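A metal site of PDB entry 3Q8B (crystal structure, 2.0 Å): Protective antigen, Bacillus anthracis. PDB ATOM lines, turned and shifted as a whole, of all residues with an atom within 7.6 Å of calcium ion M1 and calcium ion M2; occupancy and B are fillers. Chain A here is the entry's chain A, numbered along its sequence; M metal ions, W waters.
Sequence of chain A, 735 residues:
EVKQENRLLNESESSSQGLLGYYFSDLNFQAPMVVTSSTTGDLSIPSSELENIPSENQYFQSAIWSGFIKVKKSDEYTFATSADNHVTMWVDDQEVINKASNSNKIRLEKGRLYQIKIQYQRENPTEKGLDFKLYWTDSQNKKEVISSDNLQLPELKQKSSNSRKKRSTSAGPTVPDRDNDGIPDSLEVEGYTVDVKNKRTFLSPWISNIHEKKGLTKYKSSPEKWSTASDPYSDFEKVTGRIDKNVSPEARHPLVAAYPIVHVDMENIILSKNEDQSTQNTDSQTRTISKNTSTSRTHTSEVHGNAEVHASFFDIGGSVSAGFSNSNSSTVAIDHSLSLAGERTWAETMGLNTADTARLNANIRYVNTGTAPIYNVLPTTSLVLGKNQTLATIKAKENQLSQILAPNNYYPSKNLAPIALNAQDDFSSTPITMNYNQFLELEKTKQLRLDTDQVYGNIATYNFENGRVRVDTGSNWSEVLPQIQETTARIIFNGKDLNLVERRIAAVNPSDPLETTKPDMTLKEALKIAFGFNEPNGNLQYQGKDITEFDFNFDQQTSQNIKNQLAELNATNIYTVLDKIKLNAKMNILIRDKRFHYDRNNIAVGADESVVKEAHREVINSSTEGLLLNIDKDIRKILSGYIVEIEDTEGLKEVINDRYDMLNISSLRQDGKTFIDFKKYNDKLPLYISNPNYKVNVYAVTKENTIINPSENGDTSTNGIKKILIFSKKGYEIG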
ATOM      1  N   TYR A  22       1.712 -11.620  24.623  1.00  0.00           N
ATOM      2  CA  TYR A  22       0.812 -12.629  25.157  1.00  0.00           C
ATOM      3  C   TYR A  22       0.775 -12.424  26.665  1.00  0.00           C
ATOM      4  O   TYR A  22       1.819 -12.473  27.298  1.00  0.00           O
ATOM      5  CB  TYR A  22       1.323 -14.030  24.876  1.00  0.00           C
ATOM      6  CG  TYR A  22       1.402 -14.403  23.408  1.00  0.00           C
ATOM      7  CD1 TYR A  22       0.552 -13.838  22.476  1.00  0.00           C
ATOM      8  CD2 TYR A  22       2.320 -15.348  22.949  1.00  0.00           C
ATOM      9  CE1 TYR A  22       0.617 -14.166  21.137  1.00  0.00           C
ATOM     10  CE2 TYR A  22       2.385 -15.694  21.601  1.00  0.00           C
ATOM     11  CZ  TYR A  22       1.529 -15.091  20.704  1.00  0.00           C
ATOM     12  OH  TYR A  22       1.562 -15.421  19.367  1.00  0.00           O
ATOM     13  N   PRO A 176       3.734 -21.155  21.900  1.00  0.00           N
ATOM     14  CA  PRO A 176       2.550 -22.023  21.836  1.00  0.00           C
ATOM     15  C   PRO A 176       1.669 -21.612  20.617  1.00  0.00           C
ATOM     16  O   PRO A 176       0.506 -21.232  20.783  1.00  0.00           O
ATOM     17  CB  PRO A 176       1.841 -21.755  23.172  1.00  0.00           C
ATOM     18  CG  PRO A 176       2.378 -20.386  23.649  1.00  0.00           C
ATOM     19  CD  PRO A 176       3.485 -19.951  22.712  1.00  0.00           C
ATOM     20  N   ASP A 177       2.260 -21.699  19.423  1.00  0.00           N
ATOM     21  CA  ASP A 177       1.684 -21.160  18.190  1.00  0.00           C
ATOM     22  C   ASP A 177       2.117 -22.062  17.010  1.00  0.00           C
ATOM     23  O   ASP A 177       2.975 -21.704  16.208  1.00  0.00           O
ATOM     24  CB  ASP A 177       2.155 -19.711  18.002  1.00  0.00           C
ATOM     25  CG  ASP A 177       1.445 -18.989  16.846  1.00  0.00           C
ATOM     26  OD1 ASP A 177       0.509 -19.566  16.289  1.00  0.00           O
ATOM     27  OD2 ASP A 177       1.843 -17.866  16.500  1.00  0.00           O
ATOM     28  N   ARG A 178       1.524 -23.247  16.953  1.00  0.00           N
ATOM     29  CA  ARG A 178       1.961 -24.292  16.042  1.00  0.00           C
ATOM     30  C   ARG A 178       2.044 -23.802  14.613  1.00  0.00           C
ATOM     31  O   ARG A 178       2.974 -24.134  13.897  1.00  0.00           O
ATOM     32  CB  ARG A 178       1.017 -25.499  16.113  1.00  0.00           C
ATOM     33  CG  ARG A 178       1.147 -26.284  17.405  1.00  0.00           C
ATOM     34  CD  ARG A 178      -0.076 -27.122  17.685  1.00  0.00           C
ATOM     35  NE  ARG A 178       0.094 -28.482  17.227  1.00  0.00           N
ATOM     36  CZ  ARG A 178       0.865 -29.361  17.851  1.00  0.00           C
ATOM     37  NH1 ARG A 178       1.534 -28.989  18.929  1.00  0.00           N
ATOM     38  NH2 ARG A 178       0.977 -30.600  17.373  1.00  0.00           N
ATOM     39  N   ASP A 179       1.059 -23.024  14.168  1.00  0.00           N
ATOM     40  CA  ASP A 179       1.074 -22.599  12.752  1.00  0.00           C
ATOM     41  C   ASP A 179       1.738 -21.222  12.539  1.00  0.00           C
ATOM     42  O   ASP A 179       1.761 -20.699  11.429  1.00  0.00           O
ATOM     43  CB  ASP A 179      -0.353 -22.617  12.165  1.00  0.00           C
ATOM     44  CG  ASP A 179      -1.322 -21.729  12.942  1.00  0.00           C
ATOM     45  OD1 ASP A 179      -0.868 -20.812  13.646  1.00  0.00           O
ATOM     46  OD2 ASP A 179      -2.539 -21.935  12.844  1.00  0.00           O
ATOM     47  N   ASN A 180       2.260 -20.627  13.597  1.00  0.00           N
ATOM     48  CA  ASN A 180       2.928 -19.321  13.494  1.00  0.00           C
ATOM     49  C   ASN A 180       2.042 -18.200  12.943  1.00  0.00           C
ATOM     50  O   ASN A 180       2.568 -17.237  12.350  1.00  0.00           O
ATOM     51  CB  ASN A 180       4.227 -19.455  12.659  1.00  0.00           C
ATOM     52  CG  ASN A 180       5.155 -18.206  12.741  1.00  0.00           C
ATOM     53  OD1 ASN A 180       5.855 -17.904  11.779  1.00  0.00           O
ATOM     54  ND2 ASN A 180       5.146 -17.496  13.854  1.00  0.00           N
ATOM     55  N   ASP A 181       0.706 -18.233  13.154  1.00  0.00           N
ATOM     56  CA  ASP A 181      -0.053 -17.086  12.664  1.00  0.00           C
ATOM     57  C   ASP A 181      -0.064 -15.975  13.728  1.00  0.00           C
ATOM     58  O   ASP A 181      -0.462 -14.834  13.459  1.00  0.00           O
ATOM     59  CB  ASP A 181      -1.474 -17.454  12.140  1.00  0.00           C
ATOM     60  CG  ASP A 181      -2.340 -18.117  13.195  1.00  0.00           C
ATOM     61  OD1 ASP A 181      -2.135 -17.885  14.409  1.00  0.00           O
ATOM     62  OD2 ASP A 181      -3.263 -18.863  12.828  1.00  0.00           O
ATOM     63  N   GLY A 182       0.402 -16.292  14.921  1.00  0.00           N
ATOM     64  CA  GLY A 182       0.344 -15.359  16.039  1.00  0.00           C
ATOM     65  C   GLY A 182      -0.737 -15.617  17.092  1.00  0.00           C
ATOM     66  O   GLY A 182      -0.660 -15.104  18.196  1.00  0.00           O
ATOM     67  N   ILE A 183      -1.791 -16.361  16.756  1.00  0.00           N
ATOM     68  CA  ILE A 183      -2.842 -16.673  17.740  1.00  0.00           C
ATOM     69  C   ILE A 183      -2.479 -17.973  18.475  1.00  0.00           C
ATOM     70  O   ILE A 183      -2.279 -18.992  17.845  1.00  0.00           O
ATOM     71  CB  ILE A 183      -4.242 -16.868  17.061  1.00  0.00           C
ATOM     72  CG1 ILE A 183      -4.545 -15.687  16.124  1.00  0.00           C
ATOM     73  CG2 ILE A 183      -5.332 -17.066  18.125  1.00  0.00           C
ATOM     74  CD1 ILE A 183      -5.870 -15.815  15.281  1.00  0.00           C
ATOM     75  N   PRO A 184      -2.401 -17.935  19.813  1.00  0.00           N
ATOM     76  CA  PRO A 184      -2.062 -19.144  20.570  1.00  0.00           C
ATOM     77  C   PRO A 184      -2.982 -20.309  20.244  1.00  0.00           C
ATOM     78  O   PRO A 184      -4.208 -20.112  20.051  1.00  0.00           O
ATOM     79  CB  PRO A 184      -2.245 -18.734  22.048  1.00  0.00           C
ATOM     80  CG  PRO A 184      -2.070 -17.257  22.047  1.00  0.00           C
ATOM     81  CD  PRO A 184      -2.591 -16.768  20.700  1.00  0.00           C
ATOM     82  N   ASP A 185      -2.422 -21.514  20.237  1.00  0.00           N
ATOM     83  CA  ASP A 185      -3.165 -22.698  19.849  1.00  0.00           C
ATOM     84  C   ASP A 185      -4.486 -22.764  20.591  1.00  0.00           C
ATOM     85  O   ASP A 185      -5.532 -23.065  20.000  1.00  0.00           O
ATOM     86  CB  ASP A 185      -2.396 -23.987  20.137  1.00  0.00           C
ATOM     87  CG  ASP A 185      -1.015 -24.003  19.531  1.00  0.00           C
ATOM     88  OD1 ASP A 185      -0.737 -23.215  18.616  1.00  0.00           O
ATOM     89  OD2 ASP A 185      -0.187 -24.820  19.998  1.00  0.00           O
ATOM     90  N   SER A 186      -4.442 -22.502  21.890  1.00  0.00           N
ATOM     91  CA  SER A 186      -5.602 -22.801  22.739  1.00  0.00           C
ATOM     92  C   SER A 186      -6.739 -21.836  22.468  1.00  0.00           C
ATOM     93  O   SER A 186      -7.892 -22.221  22.603  1.00  0.00           O
ATOM     94  CB  SER A 186      -5.236 -22.787  24.241  1.00  0.00           C
ATOM     95  OG  SER A 186      -4.930 -21.464  24.687  1.00  0.00           O
ATOM     96  N   GLU A 188      -7.414 -20.469  19.482  1.00  0.00           N
ATOM     97  CA  GLU A 188      -7.973 -20.833  18.180  1.00  0.00           C
ATOM     98  C   GLU A 188      -8.948 -21.977  18.324  1.00  0.00           C
ATOM     99  O   GLU A 188     -10.014 -22.010  17.696  1.00  0.00           O
ATOM    100  CB  GLU A 188      -6.866 -21.229  17.231  1.00  0.00           C
ATOM    101  CG  GLU A 188      -6.104 -20.050  16.755  1.00  0.00           C
ATOM    102  CD  GLU A 188      -5.484 -20.309  15.419  1.00  0.00           C
ATOM    103  OE1 GLU A 188      -6.236 -20.336  14.390  1.00  0.00           O
ATOM    104  OE2 GLU A 188      -4.253 -20.516  15.420  1.00  0.00           O
ATOM    105  N   TYR A 192     -12.403 -17.225  20.472  1.00  0.00           N
ATOM    106  CA  TYR A 192     -11.891 -15.903  20.801  1.00  0.00           C
ATOM    107  C   TYR A 192     -12.677 -14.796  20.130  1.00  0.00           C
ATOM    108  O   TYR A 192     -13.456 -15.030  19.192  1.00  0.00           O
ATOM    109  CB  TYR A 192     -10.411 -15.791  20.385  1.00  0.00           C
ATOM    110  CG  TYR A 192     -10.116 -16.055  18.914  1.00  0.00           C
ATOM    111  CD1 TYR A 192     -10.070 -17.357  18.425  1.00  0.00           C
ATOM    112  CD2 TYR A 192      -9.818 -15.003  18.038  1.00  0.00           C
ATOM    113  CE1 TYR A 192      -9.765 -17.609  17.103  1.00  0.00           C
ATOM    114  CE2 TYR A 192      -9.524 -15.243  16.692  1.00  0.00           C
ATOM    115  CZ  TYR A 192      -9.498 -16.560  16.230  1.00  0.00           C
ATOM    116  OH  TYR A 192      -9.188 -16.862  14.917  1.00  0.00           O
ATOM    117  N   SER A 221     -10.739 -21.144  14.820  1.00  0.00           N
ATOM    118  CA  SER A 221      -9.881 -21.413  13.643  1.00  0.00           C
ATOM    119  C   SER A 221      -8.939 -22.610  13.893  1.00  0.00           C
ATOM    120  O   SER A 221      -8.785 -23.026  15.043  1.00  0.00           O
ATOM    121  CB  SER A 221      -9.108 -20.168  13.234  1.00  0.00           C
ATOM    122  OG  SER A 221      -8.674 -19.388  14.345  1.00  0.00           O
ATOM    123  N   SER A 222      -8.335 -23.193  12.866  1.00  0.00           N
ATOM    124  CA  SER A 222      -7.384 -24.287  13.115  1.00  0.00           C
ATOM    125  C   SER A 222      -6.069 -23.764  13.686  1.00  0.00           C
ATOM    126  O   SER A 222      -5.529 -22.821  13.175  1.00  0.00           O
ATOM    127  CB  SER A 222      -7.060 -25.083  11.859  1.00  0.00           C
ATOM    128  OG  SER A 222      -6.037 -26.025  12.187  1.00  0.00           O
ATOM    129  N   PRO A 223      -5.557 -24.389  14.757  1.00  0.00           N
ATOM    130  CA  PRO A 223      -4.276 -23.928  15.314  1.00  0.00           C
ATOM    131  C   PRO A 223      -3.073 -24.371  14.502  1.00  0.00           C
ATOM    132  O   PRO A 223      -1.939 -23.959  14.761  1.00  0.00           O
ATOM    133  CB  PRO A 223      -4.242 -24.567  16.730  1.00  0.00           C
ATOM    134  CG  PRO A 223      -5.088 -25.788  16.621  1.00  0.00           C
ATOM    135  CD  PRO A 223      -6.183 -25.459  15.567  1.00  0.00           C
ATOM    136  N   GLU A 224      -3.349 -25.222  13.532  1.00  0.00           N
ATOM    137  CA  GLU A 224      -2.321 -25.763  12.660  1.00  0.00           C
ATOM    138  C   GLU A 224      -2.429 -25.315  11.194  1.00  0.00           C
ATOM    139  O   GLU A 224      -1.629 -25.732  10.377  1.00  0.00           O
ATOM    140  CB  GLU A 224      -2.336 -27.282  12.767  1.00  0.00           C
ATOM    141  CG  GLU A 224      -1.977 -27.733  14.229  1.00  0.00           C
ATOM    142  CD  GLU A 224      -2.286 -29.176  14.499  1.00  0.00           C
ATOM    143  OE1 GLU A 224      -2.576 -29.516  15.678  1.00  0.00           O
ATOM    144  OE2 GLU A 224      -2.240 -29.979  13.540  1.00  0.00           O
ATOM    145  N   LYS A 225      -3.416 -24.484  10.864  1.00  0.00           N
ATOM    146  CA  LYS A 225      -3.447 -23.823   9.556  1.00  0.00           C
ATOM    147  C   LYS A 225      -3.249 -22.338   9.734  1.00  0.00           C
ATOM    148  O   LYS A 225      -4.075 -21.685  10.341  1.00  0.00           O
ATOM    149  CB  LYS A 225      -4.820 -24.031   8.881  1.00  0.00           C
ATOM    150  CG  LYS A 225      -5.130 -25.470   8.439  1.00  0.00           C
ATOM    151  CD  LYS A 225      -6.549 -25.571   7.880  1.00  0.00           C
ATOM    152  CE  LYS A 225      -6.659 -25.124   6.439  1.00  0.00           C
ATOM    153  NZ  LYS A 225      -6.072 -26.161   5.605  1.00  0.00           N
ATOM    154  N   TRP A 226      -2.194 -21.786   9.130  1.00  0.00           N
ATOM    155  CA  TRP A 226      -1.889 -20.388   9.221  1.00  0.00           C
ATOM    156  C   TRP A 226      -3.093 -19.557   8.667  1.00  0.00           C
ATOM    157  O   TRP A 226      -3.441 -18.498   9.195  1.00  0.00           O
ATOM    158  CB  TRP A 226      -0.580 -20.163   8.456  1.00  0.00           C
ATOM    159  CG  TRP A 226      -0.143 -18.774   8.315  1.00  0.00           C
ATOM    160  CD1 TRP A 226       0.634 -18.083   9.183  1.00  0.00           C
ATOM    161  CD2 TRP A 226      -0.408 -17.890   7.216  1.00  0.00           C
ATOM    162  NE1 TRP A 226       0.860 -16.814   8.704  1.00  0.00           N
ATOM    163  CE2 TRP A 226       0.242 -16.674   7.496  1.00  0.00           C
ATOM    164  CE3 TRP A 226      -1.147 -18.018   6.016  1.00  0.00           C
ATOM    165  CZ2 TRP A 226       0.177 -15.565   6.623  1.00  0.00           C
ATOM    166  CZ3 TRP A 226      -1.203 -16.918   5.159  1.00  0.00           C
ATOM    167  CH2 TRP A 226      -0.542 -15.705   5.468  1.00  0.00           C
ATOM    168  N   SER A 227      -3.718 -20.077   7.614  1.00  0.00           N
ATOM    169  CA  SER A 227      -5.002 -19.564   7.120  1.00  0.00           C
ATOM    170  C   SER A 227      -5.934 -20.746   7.124  1.00  0.00           C
ATOM    171  O   SER A 227      -5.698 -21.730   6.408  1.00  0.00           O
ATOM    172  CB  SER A 227      -4.879 -19.006   5.694  1.00  0.00           C
ATOM    173  OG  SER A 227      -6.187 -18.697   5.156  1.00  0.00           O
ATOM    174  N   THR A 228      -6.951 -20.668   7.974  1.00  0.00           N
ATOM    175  CA  THR A 228      -7.855 -21.790   8.143  1.00  0.00           C
ATOM    176  C   THR A 228      -8.689 -22.015   6.866  1.00  0.00           C
ATOM    177  O   THR A 228      -9.031 -23.146   6.526  1.00  0.00           O
ATOM    178  CB  THR A 228      -8.713 -21.575   9.403  1.00  0.00           C
ATOM    179  OG1 THR A 228      -7.842 -21.632  10.552  1.00  0.00           O
ATOM    180  CG2 THR A 228      -9.803 -22.632   9.527  1.00  0.00           C
ATOM    181  N   SER A 234      -3.556 -14.666   6.799  1.00  0.00           N
ATOM    182  CA  SER A 234      -3.571 -15.473   8.017  1.00  0.00           C
ATOM    183  C   SER A 234      -4.771 -15.210   8.956  1.00  0.00           C
ATOM    184  O   SER A 234      -5.405 -14.140   8.917  1.00  0.00           O
ATOM    185  CB  SER A 234      -2.242 -15.284   8.790  1.00  0.00           C
ATOM    186  OG  SER A 234      -2.436 -14.482   9.934  1.00  0.00           O
ATOM    187  N   ASP A 235      -5.099 -16.170   9.808  1.00  0.00           N
ATOM    188  CA  ASP A 235      -6.266 -16.011  10.688  1.00  0.00           C
ATOM    189  C   ASP A 235      -6.056 -14.765  11.550  1.00  0.00           C
ATOM    190  O   ASP A 235      -6.983 -14.060  11.927  1.00  0.00           O
ATOM    191  CB  ASP A 235      -6.422 -17.236  11.600  1.00  0.00           C
ATOM    192  CG  ASP A 235      -6.573 -18.511  10.816  1.00  0.00           C
ATOM    193  OD1 ASP A 235      -7.059 -18.466   9.665  1.00  0.00           O
ATOM    194  OD2 ASP A 235      -6.254 -19.570  11.352  1.00  0.00           O
ATOM    195  N   PHE A 236      -4.801 -14.506  11.891  1.00  0.00           N
ATOM    196  CA  PHE A 236      -4.470 -13.357  12.728  1.00  0.00           C
ATOM    197  C   PHE A 236      -4.498 -12.031  11.938  1.00  0.00           C
ATOM    198  O   PHE A 236      -5.001 -11.025  12.429  1.00  0.00           O
ATOM    199  CB  PHE A 236      -3.105 -13.598  13.396  1.00  0.00           C
ATOM    200  CG  PHE A 236      -2.607 -12.445  14.213  1.00  0.00           C
ATOM    201  CD1 PHE A 236      -3.064 -12.242  15.512  1.00  0.00           C
ATOM    202  CD2 PHE A 236      -1.632 -11.591  13.696  1.00  0.00           C
ATOM    203  CE1 PHE A 236      -2.563 -11.168  16.286  1.00  0.00           C
ATOM    204  CE2 PHE A 236      -1.136 -10.522  14.458  1.00  0.00           C
ATOM    205  CZ  PHE A 236      -1.597 -10.314  15.749  1.00  0.00           C
ATOM    206  N   PRO A 254     -11.976 -15.875   9.798  1.00  0.00           N
ATOM    207  CA  PRO A 254     -10.993 -16.905   9.459  1.00  0.00           C
ATOM    208  C   PRO A 254     -11.628 -18.118   8.792  1.00  0.00           C
ATOM    209  O   PRO A 254     -10.882 -18.915   8.261  1.00  0.00           O
ATOM    210  CB  PRO A 254     -10.383 -17.284  10.819  1.00  0.00           C
ATOM    211  CG  PRO A 254     -10.558 -16.090  11.675  1.00  0.00           C
ATOM    212  CD  PRO A 254     -11.869 -15.428  11.199  1.00  0.00           C
HETATM  213 CA    CA M   1      -4.602 -20.644  12.555  1.00  0.00          CA
HETATM  214 CA    CA M   2      -1.917 -20.055  15.728  1.00  0.00          CA
HETATM  215  O   HOH W   1      -1.676 -22.262  16.546  1.00  0.00           O
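The side-chain carboxylate of Asp 177 sits close to the backbone NH of Asn 180, at 3.4 Å. O of Glu 188 is in hydrogen-bond range of N of Ser 221, 3.1 Å away. N of Asp 235 lies within hydrogen-bond range of O of Trp 226, 2.9 Å away. The side-chain carboxylate (OD2) of Asp 179 sits close to the backbone NH (N) of Glu 224 (3.5 Å). The side-chain carboxylate (OD1) of Asp 185 lies close to the backbone NH (N) of Asp 177 (3.5 Å). N of Ser 222 lies within hydrogen-bond range of OG1 of Thr 228 (2.8 Å). The side-chain hydroxyl (OG) of Ser 222 sits at hydrogen-bond distance from the backbone NH (N) of Lys 225 (3.3 Å). The side-chain carboxylate of Asp 235 lies within hydrogen-bond range of the backbone NH of Thr 228 (2.8 Å).
Residues that only touch calcium ion M1: Thr 228. Within 4 Å of calcium ion M1: Asp 179, Asp 181, Glu 188, Ser 222, Lys 225, Thr 228 and Asp 235.
Within 4 Å of calcium ion M2: Asp 177, Asp 179, Asp 181, Ile 183 and Glu 188. The nearest printed residue that does not touch calcium ion M2 is Pro 223 (4.02 Å).
Calcium ion M1 is bound by the side-chain carboxylate (OD2) of Asp 181. OD2 of Asp 235 is bound to calcium ion M1, 2.3 Å away. Calcium ion M1 is bound by the backbone carbonyl oxygen (O) of Ser 222. OD2 of Asp 179 binds calcium ion M1 (2.5 Å). OE1 of Glu 188 is bound to calcium ion M1, at 2.5 Å. O of Lys 225 binds calcium ion M1. OE2 of Glu 188 binds calcium ion M1, at 2.9 Å. Calcium ion M1 has seven donor atoms within binding distance.
Water W1 is bound to calcium ion M2. O of Ile 183 is bound to calcium ion M2. OE2 of Glu 188 is bound to calcium ion M2, 2.4 Å away. OD1 of Asp 179 binds calcium ion M2 (2.5 Å). OD1 of Asp 177 binds calcium ion M2 (2.5 Å). OD1 of Asp 181 is bound to calcium ion M2 (2.5 Å).
Water W1 lies within hydrogen-bond range of OD1 of Asp 185 (2.5 Å), O of Pro 223 (2.5 Å) and N of Arg 178 (3.4 Å).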
